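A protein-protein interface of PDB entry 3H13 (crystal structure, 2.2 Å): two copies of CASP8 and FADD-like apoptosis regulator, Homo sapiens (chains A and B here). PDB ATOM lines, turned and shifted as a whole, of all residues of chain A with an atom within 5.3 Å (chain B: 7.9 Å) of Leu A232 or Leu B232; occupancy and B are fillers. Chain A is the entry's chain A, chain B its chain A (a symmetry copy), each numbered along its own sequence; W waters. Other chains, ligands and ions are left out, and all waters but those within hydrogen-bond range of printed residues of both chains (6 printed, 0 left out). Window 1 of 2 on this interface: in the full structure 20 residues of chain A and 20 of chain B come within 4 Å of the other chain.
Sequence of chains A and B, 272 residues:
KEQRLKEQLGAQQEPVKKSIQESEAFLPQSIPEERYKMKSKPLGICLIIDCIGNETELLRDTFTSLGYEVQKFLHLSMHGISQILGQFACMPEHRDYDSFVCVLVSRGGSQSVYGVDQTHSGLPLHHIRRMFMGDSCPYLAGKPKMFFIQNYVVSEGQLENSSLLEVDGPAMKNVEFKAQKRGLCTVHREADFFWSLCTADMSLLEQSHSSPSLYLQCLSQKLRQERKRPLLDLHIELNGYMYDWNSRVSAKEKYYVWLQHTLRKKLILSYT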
ATOM      1  N   PHE A 194      12.018 -26.249   6.511  1.00  0.00           N
ATOM      2  CA  PHE A 194      12.669 -24.969   6.790  1.00  0.00           C
ATOM      3  C   PHE A 194      13.963 -25.433   7.475  1.00  0.00           C
ATOM      4  O   PHE A 194      13.941 -26.091   8.531  1.00  0.00           O
ATOM      5  CB  PHE A 194      11.844 -24.102   7.736  1.00  0.00           C
ATOM      6  CG  PHE A 194      12.433 -22.731   7.973  1.00  0.00           C
ATOM      7  CD1 PHE A 194      12.075 -21.654   7.172  1.00  0.00           C
ATOM      8  CD2 PHE A 194      13.348 -22.518   9.001  1.00  0.00           C
ATOM      9  CE1 PHE A 194      12.622 -20.371   7.395  1.00  0.00           C
ATOM     10  CE2 PHE A 194      13.896 -21.248   9.226  1.00  0.00           C
ATOM     11  CZ  PHE A 194      13.528 -20.177   8.420  1.00  0.00           C
ATOM     12  N   PRO A 230       6.185 -13.255   9.927  1.00  0.00           N
ATOM     13  CA  PRO A 230       6.553 -14.556   9.374  1.00  0.00           C
ATOM     14  C   PRO A 230       7.984 -14.976   9.715  1.00  0.00           C
ATOM     15  O   PRO A 230       8.893 -14.143   9.827  1.00  0.00           O
ATOM     16  CB  PRO A 230       6.288 -14.405   7.869  1.00  0.00           C
ATOM     17  CG  PRO A 230       5.969 -12.956   7.657  1.00  0.00           C
ATOM     18  CD  PRO A 230       5.489 -12.411   8.941  1.00  0.00           C
ATOM     19  N   LEU A 231       8.173 -16.277   9.906  1.00  0.00           N
ATOM     20  CA  LEU A 231       9.479 -16.803  10.269  1.00  0.00           C
ATOM     21  C   LEU A 231      10.561 -16.346   9.289  1.00  0.00           C
ATOM     22  O   LEU A 231      11.650 -15.957   9.701  1.00  0.00           O
ATOM     23  CB  LEU A 231       9.438 -18.338  10.321  1.00  0.00           C
ATOM     24  CG  LEU A 231      10.777 -19.025  10.622  1.00  0.00           C
ATOM     25  CD1 LEU A 231      11.256 -18.593  12.004  1.00  0.00           C
ATOM     26  CD2 LEU A 231      10.611 -20.547  10.559  1.00  0.00           C
ATOM     27  N   LEU A 232      10.240 -16.381   7.998  1.00  0.00           N
ATOM     28  CA  LEU A 232      11.172 -15.988   6.949  1.00  0.00           C
ATOM     29  C   LEU A 232      11.645 -14.537   7.085  1.00  0.00           C
ATOM     30  O   LEU A 232      12.824 -14.245   6.865  1.00  0.00           O
ATOM     31  CB  LEU A 232      10.512 -16.189   5.591  1.00  0.00           C
ATOM     32  CG  LEU A 232      11.420 -16.424   4.392  1.00  0.00           C
ATOM     33  CD1 LEU A 232      12.446 -17.503   4.763  1.00  0.00           C
ATOM     34  CD2 LEU A 232      10.575 -16.899   3.181  1.00  0.00           C
ATOM     35  N   ASP A 233      10.727 -13.633   7.429  1.00  0.00           N
ATOM     36  CA  ASP A 233      11.078 -12.224   7.607  1.00  0.00           C
ATOM     37  C   ASP A 233      11.992 -12.044   8.821  1.00  0.00           C
ATOM     38  O   ASP A 233      12.901 -11.195   8.805  1.00  0.00           O
ATOM     39  CB  ASP A 233       9.823 -11.367   7.792  1.00  0.00           C
ATOM     40  CG  ASP A 233       8.956 -11.317   6.538  1.00  0.00           C
ATOM     41  OD1 ASP A 233       9.440 -11.718   5.463  1.00  0.00           O
ATOM     42  OD2 ASP A 233       7.802 -10.859   6.618  1.00  0.00           O
ATOM     43  N   LEU A 234      11.751 -12.835   9.870  1.00  0.00           N
ATOM     44  CA  LEU A 234      12.577 -12.758  11.092  1.00  0.00           C
ATOM     45  C   LEU A 234      13.964 -13.268  10.744  1.00  0.00           C
ATOM     46  O   LEU A 234      14.971 -12.724  11.176  1.00  0.00           O
ATOM     47  CB  LEU A 234      11.983 -13.627  12.224  1.00  0.00           C
ATOM     48  CG  LEU A 234      10.607 -13.171  12.756  1.00  0.00           C
ATOM     49  CD1 LEU A 234      10.096 -14.152  13.803  1.00  0.00           C
ATOM     50  CD2 LEU A 234      10.720 -11.769  13.337  1.00  0.00           C
ATOM     51  N   HIS A 235      14.014 -14.314   9.935  1.00  0.00           N
ATOM     52  CA  HIS A 235      15.298 -14.869   9.565  1.00  0.00           C
ATOM     53  C   HIS A 235      16.114 -13.890   8.708  1.00  0.00           C
ATOM     54  O   HIS A 235      17.342 -13.880   8.790  1.00  0.00           O
ATOM     55  CB  HIS A 235      15.108 -16.206   8.854  1.00  0.00           C
ATOM     56  CG  HIS A 235      16.286 -17.118   8.989  1.00  0.00           C
ATOM     57  ND1 HIS A 235      17.435 -16.966   8.243  1.00  0.00           N
ATOM     58  CD2 HIS A 235      16.495 -18.188   9.792  1.00  0.00           C
ATOM     59  CE1 HIS A 235      18.299 -17.913   8.572  1.00  0.00           C
ATOM     60  NE2 HIS A 235      17.753 -18.670   9.508  1.00  0.00           N
ATOM     61  N   ILE A 236      15.438 -13.062   7.910  1.00  0.00           N
ATOM     62  CA  ILE A 236      16.118 -12.043   7.076  1.00  0.00           C
ATOM     63  C   ILE A 236      16.799 -11.040   8.019  1.00  0.00           C
ATOM     64  O   ILE A 236      17.955 -10.657   7.812  1.00  0.00           O
ATOM     65  CB  ILE A 236      15.122 -11.235   6.203  1.00  0.00           C
ATOM     66  CG1 ILE A 236      14.555 -12.103   5.083  1.00  0.00           C
ATOM     67  CG2 ILE A 236      15.807  -9.974   5.641  1.00  0.00           C
ATOM     68  CD1 ILE A 236      15.572 -12.643   4.169  1.00  0.00           C
ATOM     69  N   LEU A 259      20.516 -20.657   4.864  1.00  0.00           N
ATOM     70  CA  LEU A 259      19.092 -20.972   4.908  1.00  0.00           C
ATOM     71  C   LEU A 259      18.602 -21.597   3.604  1.00  0.00           C
ATOM     72  O   LEU A 259      18.852 -21.085   2.504  1.00  0.00           O
ATOM     73  CB  LEU A 259      18.249 -19.730   5.220  1.00  0.00           C
ATOM     74  CG  LEU A 259      16.730 -19.952   5.065  1.00  0.00           C
ATOM     75  CD1 LEU A 259      16.187 -20.899   6.152  1.00  0.00           C
ATOM     76  CD2 LEU A 259      16.028 -18.596   5.130  1.00  0.00           C
ATOM     77  N   HIS A 261      14.893 -23.588   2.214  1.00  0.00           N
ATOM     78  CA  HIS A 261      13.544 -24.021   2.560  1.00  0.00           C
ATOM     79  C   HIS A 261      12.689 -24.398   1.342  1.00  0.00           C
ATOM     80  O   HIS A 261      13.029 -24.085   0.188  1.00  0.00           O
ATOM     81  CB  HIS A 261      12.834 -22.971   3.426  1.00  0.00           C
ATOM     82  CG  HIS A 261      12.377 -21.766   2.673  1.00  0.00           C
ATOM     83  ND1 HIS A 261      11.219 -21.754   1.925  1.00  0.00           N
ATOM     84  CD2 HIS A 261      12.933 -20.538   2.530  1.00  0.00           C
ATOM     85  CE1 HIS A 261      11.079 -20.572   1.353  1.00  0.00           C
ATOM     86  NE2 HIS A 261      12.105 -19.815   1.702  1.00  0.00           N
ATOM     87  N   LEU A 263       9.105 -24.040   1.696  1.00  0.00           N
ATOM     88  CA  LEU A 263       7.797 -23.607   2.159  1.00  0.00           C
ATOM     89  C   LEU A 263       6.913 -23.303   0.963  1.00  0.00           C
ATOM     90  O   LEU A 263       7.402 -22.838  -0.071  1.00  0.00           O
ATOM     91  CB  LEU A 263       7.915 -22.362   3.030  1.00  0.00           C
ATOM     92  CG  LEU A 263       8.705 -22.602   4.317  1.00  0.00           C
ATOM     93  CD1 LEU A 263       8.625 -21.348   5.204  1.00  0.00           C
ATOM     94  CD2 LEU A 263       8.143 -23.852   5.025  1.00  0.00           C
ATOM     95  N   LEU A 267       4.537 -18.739   6.602  1.00  0.00           N
ATOM     96  CA  LEU A 267       4.692 -19.417   7.885  1.00  0.00           C
ATOM     97  C   LEU A 267       4.881 -18.453   9.057  1.00  0.00           C
ATOM     98  O   LEU A 267       5.883 -17.720   9.150  1.00  0.00           O
ATOM     99  CB  LEU A 267       5.872 -20.389   7.803  1.00  0.00           C
ATOM    100  CG  LEU A 267       6.256 -21.081   9.113  1.00  0.00           C
ATOM    101  CD1 LEU A 267       5.019 -21.860   9.655  1.00  0.00           C
ATOM    102  CD2 LEU A 267       7.430 -22.030   8.877  1.00  0.00           C
ATOM    103  N   PHE B 194      20.000 -12.638  -4.516  1.00  0.00           N
ATOM    104  CA  PHE B 194      18.744 -13.385  -4.575  1.00  0.00           C
ATOM    105  C   PHE B 194      18.978 -14.265  -5.812  1.00  0.00           C
ATOM    106  O   PHE B 194      19.184 -13.769  -6.935  1.00  0.00           O
ATOM    107  CB  PHE B 194      17.543 -12.471  -4.789  1.00  0.00           C
ATOM    108  CG  PHE B 194      16.216 -13.193  -4.759  1.00  0.00           C
ATOM    109  CD1 PHE B 194      15.507 -13.332  -3.573  1.00  0.00           C
ATOM    110  CD2 PHE B 194      15.675 -13.734  -5.922  1.00  0.00           C
ATOM    111  CE1 PHE B 194      14.265 -14.004  -3.544  1.00  0.00           C
ATOM    112  CE2 PHE B 194      14.444 -14.404  -5.900  1.00  0.00           C
ATOM    113  CZ  PHE B 194      13.743 -14.535  -4.708  1.00  0.00           C
ATOM    114  N   LEU B 223       5.009 -11.122 -10.241  1.00  0.00           N
ATOM    115  CA  LEU B 223       5.645  -9.807 -10.153  1.00  0.00           C
ATOM    116  C   LEU B 223       4.793  -8.714 -10.772  1.00  0.00           C
ATOM    117  O   LEU B 223       4.687  -7.614 -10.226  1.00  0.00           O
ATOM    118  CB  LEU B 223       7.027  -9.825 -10.803  1.00  0.00           C
ATOM    119  CG  LEU B 223       8.055 -10.625  -9.999  1.00  0.00           C
ATOM    120  CD1 LEU B 223       9.396 -10.707 -10.733  1.00  0.00           C
ATOM    121  CD2 LEU B 223       8.226  -9.959  -8.652  1.00  0.00           C
ATOM    122  N   ARG B 229       3.915  -6.881  -2.931  1.00  0.00           N
ATOM    123  CA  ARG B 229       4.275  -7.885  -1.936  1.00  0.00           C
ATOM    124  C   ARG B 229       5.772  -8.180  -2.028  1.00  0.00           C
ATOM    125  O   ARG B 229       6.371  -8.043  -3.086  1.00  0.00           O
ATOM    126  CB  ARG B 229       3.444  -9.143  -2.156  1.00  0.00           C
ATOM    127  CG  ARG B 229       1.948  -8.840  -2.040  1.00  0.00           C
ATOM    128  CD  ARG B 229       1.133 -10.047  -2.439  1.00  0.00           C
ATOM    129  NE  ARG B 229       1.584 -11.189  -1.663  1.00  0.00           N
ATOM    130  CZ  ARG B 229       1.139 -12.425  -1.820  1.00  0.00           C
ATOM    131  NH1 ARG B 229       0.211 -12.693  -2.739  1.00  0.00           N
ATOM    132  NH2 ARG B 229       1.636 -13.393  -1.056  1.00  0.00           N
ATOM    133  N   PRO B 230       6.406  -8.549  -0.907  1.00  0.00           N
ATOM    134  CA  PRO B 230       7.837  -8.829  -1.004  1.00  0.00           C
ATOM    135  C   PRO B 230       8.167  -9.958  -1.982  1.00  0.00           C
ATOM    136  O   PRO B 230       7.401 -10.917  -2.145  1.00  0.00           O
ATOM    137  CB  PRO B 230       8.256  -9.115   0.445  1.00  0.00           C
ATOM    138  CG  PRO B 230       6.981  -9.163   1.233  1.00  0.00           C
ATOM    139  CD  PRO B 230       5.966  -8.394   0.491  1.00  0.00           C
ATOM    140  N   LEU B 231       9.306  -9.824  -2.653  1.00  0.00           N
ATOM    141  CA  LEU B 231       9.720 -10.811  -3.638  1.00  0.00           C
ATOM    142  C   LEU B 231       9.724 -12.224  -3.051  1.00  0.00           C
ATOM    143  O   LEU B 231       9.263 -13.165  -3.691  1.00  0.00           O
ATOM    144  CB  LEU B 231      11.116 -10.467  -4.179  1.00  0.00           C
ATOM    145  CG  LEU B 231      11.704 -11.475  -5.177  1.00  0.00           C
ATOM    146  CD1 LEU B 231      10.803 -11.536  -6.407  1.00  0.00           C
ATOM    147  CD2 LEU B 231      13.125 -11.057  -5.569  1.00  0.00           C
ATOM    148  N   LEU B 232      10.231 -12.352  -1.826  1.00  0.00           N
ATOM    149  CA  LEU B 232      10.314 -13.637  -1.145  1.00  0.00           C
ATOM    150  C   LEU B 232       8.946 -14.301  -0.957  1.00  0.00           C
ATOM    151  O   LEU B 232       8.818 -15.517  -1.117  1.00  0.00           O
ATOM    152  CB  LEU B 232      10.982 -13.442   0.211  1.00  0.00           C
ATOM    153  CG  LEU B 232      11.700 -14.638   0.821  1.00  0.00           C
ATOM    154  CD1 LEU B 232      12.607 -15.259  -0.249  1.00  0.00           C
ATOM    155  CD2 LEU B 232      12.556 -14.173   2.028  1.00  0.00           C
ATOM    156  N   ASP B 233       7.933 -13.507  -0.604  1.00  0.00           N
ATOM    157  CA  ASP B 233       6.582 -14.037  -0.419  1.00  0.00           C
ATOM    158  C   ASP B 233       6.000 -14.509  -1.754  1.00  0.00           C
ATOM    159  O   ASP B 233       5.269 -15.514  -1.802  1.00  0.00           O
ATOM    160  CB  ASP B 233       5.656 -12.977   0.184  1.00  0.00           C
ATOM    161  CG  ASP B 233       6.043 -12.604   1.612  1.00  0.00           C
ATOM    162  OD1 ASP B 233       6.847 -13.335   2.221  1.00  0.00           O
ATOM    163  OD2 ASP B 233       5.532 -11.597   2.134  1.00  0.00           O
ATOM    164  N   LEU B 234       6.320 -13.788  -2.832  1.00  0.00           N
ATOM    165  CA  LEU B 234       5.827 -14.157  -4.173  1.00  0.00           C
ATOM    166  C   LEU B 234       6.500 -15.459  -4.570  1.00  0.00           C
ATOM    167  O   LEU B 234       5.885 -16.347  -5.144  1.00  0.00           O
ATOM    168  CB  LEU B 234       6.170 -13.067  -5.216  1.00  0.00           C
ATOM    169  CG  LEU B 234       5.477 -11.704  -4.999  1.00  0.00           C
ATOM    170  CD1 LEU B 234       5.960 -10.698  -6.036  1.00  0.00           C
ATOM    171  CD2 LEU B 234       3.967 -11.878  -5.075  1.00  0.00           C
ATOM    172  N   HIS B 235       7.777 -15.579  -4.241  1.00  0.00           N
ATOM    173  CA  HIS B 235       8.494 -16.784  -4.595  1.00  0.00           C
ATOM    174  C   HIS B 235       7.957 -18.008  -3.839  1.00  0.00           C
ATOM    175  O   HIS B 235       7.978 -19.117  -4.373  1.00  0.00           O
ATOM    176  CB  HIS B 235       9.989 -16.595  -4.357  1.00  0.00           C
ATOM    177  CG  HIS B 235      10.840 -17.466  -5.224  1.00  0.00           C
ATOM    178  ND1 HIS B 235      11.041 -18.805  -4.967  1.00  0.00           N
ATOM    179  CD2 HIS B 235      11.534 -17.190  -6.354  1.00  0.00           C
ATOM    180  CE1 HIS B 235      11.834 -19.315  -5.895  1.00  0.00           C
ATOM    181  NE2 HIS B 235      12.150 -18.357  -6.747  1.00  0.00           N
ATOM    182  N   ILE B 236       7.461 -17.805  -2.617  1.00  0.00           N
ATOM    183  CA  ILE B 236       6.871 -18.903  -1.815  1.00  0.00           C
ATOM    184  C   ILE B 236       5.619 -19.406  -2.553  1.00  0.00           C
ATOM    185  O   ILE B 236       5.403 -20.614  -2.685  1.00  0.00           O
ATOM    186  CB  ILE B 236       6.405 -18.427  -0.414  1.00  0.00           C
ATOM    187  CG1 ILE B 236       7.604 -18.114   0.478  1.00  0.00           C
ATOM    188  CG2 ILE B 236       5.489 -19.484   0.233  1.00  0.00           C
ATOM    189  CD1 ILE B 236       8.501 -19.258   0.700  1.00  0.00           C
ATOM    190  N   GLU B 237       4.797 -18.466  -3.016  1.00  0.00           N
ATOM    191  CA  GLU B 237       3.591 -18.819  -3.775  1.00  0.00           C
ATOM    192  C   GLU B 237       4.008 -19.504  -5.070  1.00  0.00           C
ATOM    193  O   GLU B 237       3.367 -20.464  -5.491  1.00  0.00           O
ATOM    194  CB  GLU B 237       2.765 -17.575  -4.075  1.00  0.00           C
ATOM    195  CG  GLU B 237       2.486 -16.772  -2.814  1.00  0.00           C
ATOM    196  CD  GLU B 237       1.462 -15.680  -3.026  1.00  0.00           C
ATOM    197  OE1 GLU B 237       1.454 -15.053  -4.105  1.00  0.00           O
ATOM    198  OE2 GLU B 237       0.662 -15.452  -2.097  1.00  0.00           O
ATOM    199  N   LEU B 238       5.078 -19.027  -5.704  1.00  0.00           N
ATOM    200  CA  LEU B 238       5.540 -19.694  -6.925  1.00  0.00           C
ATOM    201  C   LEU B 238       5.932 -21.145  -6.581  1.00  0.00           C
ATOM    202  O   LEU B 238       5.620 -22.050  -7.349  1.00  0.00           O
ATOM    203  CB  LEU B 238       6.727 -18.953  -7.544  1.00  0.00           C
ATOM    204  CG  LEU B 238       7.330 -19.521  -8.839  1.00  0.00           C
ATOM    205  CD1 LEU B 238       7.929 -18.379  -9.662  1.00  0.00           C
ATOM    206  CD2 LEU B 238       8.402 -20.534  -8.520  1.00  0.00           C
ATOM    207  N   ASN B 239       6.581 -21.356  -5.424  1.00  0.00           N
ATOM    208  CA  ASN B 239       6.984 -22.710  -4.964  1.00  0.00           C
ATOM    209  C   ASN B 239       5.730 -23.589  -4.931  1.00  0.00           C
ATOM    210  O   ASN B 239       5.715 -24.676  -5.485  1.00  0.00           O
ATOM    211  CB  ASN B 239       7.519 -22.732  -3.515  1.00  0.00           C
ATOM    212  CG  ASN B 239       8.941 -22.252  -3.378  1.00  0.00           C
ATOM    213  OD1 ASN B 239       9.648 -22.036  -4.373  1.00  0.00           O
ATOM    214  ND2 ASN B 239       9.392 -22.096  -2.106  1.00  0.00           N
ATOM    215  N   LEU B 259      15.889 -22.087  -4.454  1.00  0.00           N
ATOM    216  CA  LEU B 259      16.091 -20.698  -4.056  1.00  0.00           C
ATOM    217  C   LEU B 259      17.140 -20.564  -2.955  1.00  0.00           C
ATOM    218  O   LEU B 259      17.097 -21.258  -1.930  1.00  0.00           O
ATOM    219  CB  LEU B 259      14.783 -20.048  -3.591  1.00  0.00           C
ATOM    220  CG  LEU B 259      14.971 -18.655  -2.954  1.00  0.00           C
ATOM    221  CD1 LEU B 259      15.405 -17.613  -4.002  1.00  0.00           C
ATOM    222  CD2 LEU B 259      13.658 -18.239  -2.291  1.00  0.00           C
ATOM    223  N   GLN B 260      18.082 -19.656  -3.185  1.00  0.00           N
ATOM    224  CA  GLN B 260      19.137 -19.369  -2.237  1.00  0.00           C
ATOM    225  C   GLN B 260      19.277 -17.837  -2.199  1.00  0.00           C
ATOM    226  O   GLN B 260      19.307 -17.205  -3.260  1.00  0.00           O
ATOM    227  CB  GLN B 260      20.433 -20.011  -2.743  1.00  0.00           C
ATOM    228  CG  GLN B 260      21.492 -20.251  -1.692  1.00  0.00           C
ATOM    229  CD  GLN B 260      21.007 -21.171  -0.573  1.00  0.00           C
ATOM    230  OE1 GLN B 260      20.232 -22.105  -0.810  1.00  0.00           O
ATOM    231  NE2 GLN B 260      21.465 -20.910   0.650  1.00  0.00           N
ATOM    232  N   HIS B 261      19.320 -17.228  -1.012  1.00  0.00           N
ATOM    233  CA  HIS B 261      19.519 -15.785  -0.943  1.00  0.00           C
ATOM    234  C   HIS B 261      20.287 -15.331   0.308  1.00  0.00           C
ATOM    235  O   HIS B 261      20.454 -16.090   1.278  1.00  0.00           O
ATOM    236  CB  HIS B 261      18.184 -15.037  -1.069  1.00  0.00           C
ATOM    237  CG  HIS B 261      17.335 -15.093   0.157  1.00  0.00           C
ATOM    238  ND1 HIS B 261      17.549 -14.275   1.247  1.00  0.00           N
ATOM    239  CD2 HIS B 261      16.283 -15.884   0.479  1.00  0.00           C
ATOM    240  CE1 HIS B 261      16.668 -14.558   2.187  1.00  0.00           C
ATOM    241  NE2 HIS B 261      15.888 -15.532   1.749  1.00  0.00           N
ATOM    242  N   LEU B 263      19.642 -11.970   1.483  1.00  0.00           N
ATOM    243  CA  LEU B 263      19.000 -10.688   1.725  1.00  0.00           C
ATOM    244  C   LEU B 263      19.129 -10.328   3.194  1.00  0.00           C
ATOM    245  O   LEU B 263      19.117 -11.212   4.055  1.00  0.00           O
ATOM    246  CB  LEU B 263      17.525 -10.740   1.344  1.00  0.00           C
ATOM    247  CG  LEU B 263      17.298 -10.994  -0.146  1.00  0.00           C
ATOM    248  CD1 LEU B 263      15.799 -10.861  -0.462  1.00  0.00           C
ATOM    249  CD2 LEU B 263      18.155 -10.004  -0.961  1.00  0.00           C
ATOM    250  N   LYS B 265      17.344  -7.358   4.235  1.00  0.00           N
ATOM    251  CA  LYS B 265      16.209  -6.489   4.488  1.00  0.00           C
ATOM    252  C   LYS B 265      15.051  -6.968   3.640  1.00  0.00           C
ATOM    253  O   LYS B 265      15.231  -7.769   2.718  1.00  0.00           O
ATOM    254  CB  LYS B 265      16.520  -5.040   4.072  1.00  0.00           C
ATOM    255  CG  LYS B 265      17.847  -4.466   4.566  1.00  0.00           C
ATOM    256  CD  LYS B 265      18.003  -3.019   4.087  1.00  0.00           C
ATOM    257  CE  LYS B 265      19.390  -2.472   4.411  1.00  0.00           C
ATOM    258  NZ  LYS B 265      19.598  -1.111   3.836  1.00  0.00           N
ATOM    259  N   LYS B 266      13.863  -6.466   3.941  1.00  0.00           N
ATOM    260  CA  LYS B 266      12.700  -6.825   3.170  1.00  0.00           C
ATOM    261  C   LYS B 266      12.873  -6.260   1.750  1.00  0.00           C
ATOM    262  O   LYS B 266      13.192  -5.078   1.558  1.00  0.00           O
ATOM    263  CB  LYS B 266      11.453  -6.248   3.808  1.00  0.00           C
ATOM    264  CG  LYS B 266      10.205  -6.465   2.962  1.00  0.00           C
ATOM    265  CD  LYS B 266       8.947  -6.364   3.794  1.00  0.00           C
ATOM    266  CE  LYS B 266       8.913  -7.490   4.806  1.00  0.00           C
ATOM    267  NZ  LYS B 266       7.574  -7.609   5.411  1.00  0.00           N
ATOM    268  N   LEU B 267      12.652  -7.107   0.756  1.00  0.00           N
ATOM    269  CA  LEU B 267      12.798  -6.695  -0.636  1.00  0.00           C
ATOM    270  C   LEU B 267      11.472  -6.659  -1.397  1.00  0.00           C
ATOM    271  O   LEU B 267      10.811  -7.691  -1.613  1.00  0.00           O
ATOM    272  CB  LEU B 267      13.787  -7.629  -1.338  1.00  0.00           C
ATOM    273  CG  LEU B 267      13.948  -7.417  -2.845  1.00  0.00           C
ATOM    274  CD1 LEU B 267      14.399  -5.947  -3.103  1.00  0.00           C
ATOM    275  CD2 LEU B 267      14.973  -8.402  -3.404  1.00  0.00           C
ATOM    276  N   ILE B 268      11.081  -5.453  -1.786  1.00  0.00           N
ATOM    277  CA  ILE B 268       9.844  -5.226  -2.529  1.00  0.00           C
ATOM    278  C   ILE B 268      10.196  -4.440  -3.799  1.00  0.00           C
ATOM    279  O   ILE B 268      10.801  -3.352  -3.732  1.00  0.00           O
ATOM    280  CB  ILE B 268       8.841  -4.434  -1.674  1.00  0.00           C
ATOM    281  CG1 ILE B 268       8.463  -5.259  -0.426  1.00  0.00           C
ATOM    282  CG2 ILE B 268       7.597  -4.111  -2.491  1.00  0.00           C
ATOM    283  CD1 ILE B 268       7.607  -4.490   0.593  1.00  0.00           C
ATOM    284  N   LEU B 269       9.833  -4.998  -4.952  1.00  0.00           N
ATOM    285  CA  LEU B 269      10.149  -4.383  -6.246  1.00  0.00           C
ATOM    286  C   LEU B 269       9.201  -3.266  -6.697  1.00  0.00           C
ATOM    287  O   LEU B 269       8.572  -3.358  -7.735  1.00  0.00           O
ATOM    288  CB  LEU B 269      10.232  -5.465  -7.347  1.00  0.00           C
ATOM    289  CG  LEU B 269      11.178  -6.650  -7.094  1.00  0.00           C
ATOM    290  CD1 LEU B 269      11.467  -7.387  -8.391  1.00  0.00           C
ATOM    291  CD2 LEU B 269      12.483  -6.152  -6.505  1.00  0.00           C
HETATM  292  O   HOH W   1      15.273 -21.791  -0.129  1.00  0.00           O
HETATM  293  O   HOH W   2      14.985 -23.878  -2.478  1.00  0.00           O
HETATM  294  O   HOH W   3      12.508 -21.819  -1.550  1.00  0.00           O
HETATM  295  O   HOH W   4      18.568 -18.699   1.465  1.00  0.00           O
HETATM  296  O   HOH W   5       7.584  -8.794   8.398  1.00  0.00           O
HETATM  297  O   HOH W   6      21.374 -18.826   2.904  1.00  0.00           O
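The side-chain carboxylate (OD2) of Asp A233 is in salt-bridge range of the side-chain amino group (NZ) of Lys B266 (3.5 Å). The side-chain amide nitrogen (NE2) of Gln B260 is in hydrogen-bond range of the backbone carbonyl oxygen (O) of Leu A259. The backbone carbonyl oxygen of Leu A263 is in hydrogen-bond range of the side-chain amide nitrogen of Asn B239, 2.9 Å away.
Of the 22 printed residues of chain B, 8 touch a printed residue of chain A. Along chain B the printed residues that touch a printed residue of chain A span positions 232 to 266. Printed residues of chain A that touch a printed residue of chain B: Leu A232, Asp A233, Ile A236, Leu A259, His A261 and Leu A263. Among the printed residues, 9 pairs touch across the chains. Among the printed residues, Asp or Glu carboxylates within 4 Å of a Lys or Arg side-chain nitrogen of the other chain: Asp A233 with Lys B266 (3.5 Å).
Among the printed residues, merely in contact across the chains: Ile A236 with His B261 (3.0 Å), His A261 with Ile B236 (3.0 Å), Ile A236 with Lys B265 (3.3 Å), Leu A232 with Leu B232 (3.5 Å), Leu A263 with Ile B236 (3.8 Å) and Ile A236 with Leu B263 (3.8 Å).
Leu B232 touches its own counterpart, Leu A232. Ile A236 touches His B261, and with the chains exchanged His A261 touches Ile B236. Ile A236 touches Leu B263, and with the chains exchanged Leu A263 touches Ile B236. Positions printed for both chains: 194, 230, 231, 232, 233, 234, 235, 236, 259, 261, 263 and 267.
ND1 of His A261 lies within hydrogen-bond range of N of Leu A263, 3.1 Å away. The side-chain amide oxygen (OD1) of Asn B239 sits close to the backbone carbonyl oxygen (O) of His B235 (3.4 Å). A ring nitrogen (ND1) of His B261 sits at hydrogen-bond distance from the backbone NH (N) of Leu B263 (3.1 Å).
Printed residues of chain B within 4 Å of Leu A232: Leu B232 (3.5 Å). Of the printed residues of chain A, Leu B232 touches Leu A232. Printed residues of chain B within 4 Å of Leu A259: Gln B260. Printed residues of chain A within 4 Å of Gln B260: Leu A259 (3.2 Å). Printed residues of chain B within 4 Å of His A261: Ile B236 (3.0 Å). Asp B233 touches none of the printed residues of chain A. The nearest printed residue of chain B that does not touch Leu A232 is Ile B236 (4.003 Å).
Water W1 bridges O of Leu B259 (2.6 Å) and N of His A261 (3.0 Å). Water W4 bridges the backbone carbonyl oxygen (O) of Leu A259 (2.6 Å) and the backbone NH (N) of His B261 (3.0 Å). Water W5 bridges OD2 of Asp A233 (2.7 Å) and NZ of Lys B266 (3.2 Å). Water W2 lies within hydrogen-bond range of the backbone NH (N) of Leu B259 and the backbone carbonyl oxygen (O) of His A261. Water W6 lies within hydrogen-bond range of N of Leu A259 (2.8 Å), NE2 of Gln B260 (3.1 Å) and O of His B261 (3.3 Å). Water W3 bridges the backbone carbonyl oxygen of His A261 (2.9 Å) and the side-chain amide nitrogen of Asn B239 (3.2 Å).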
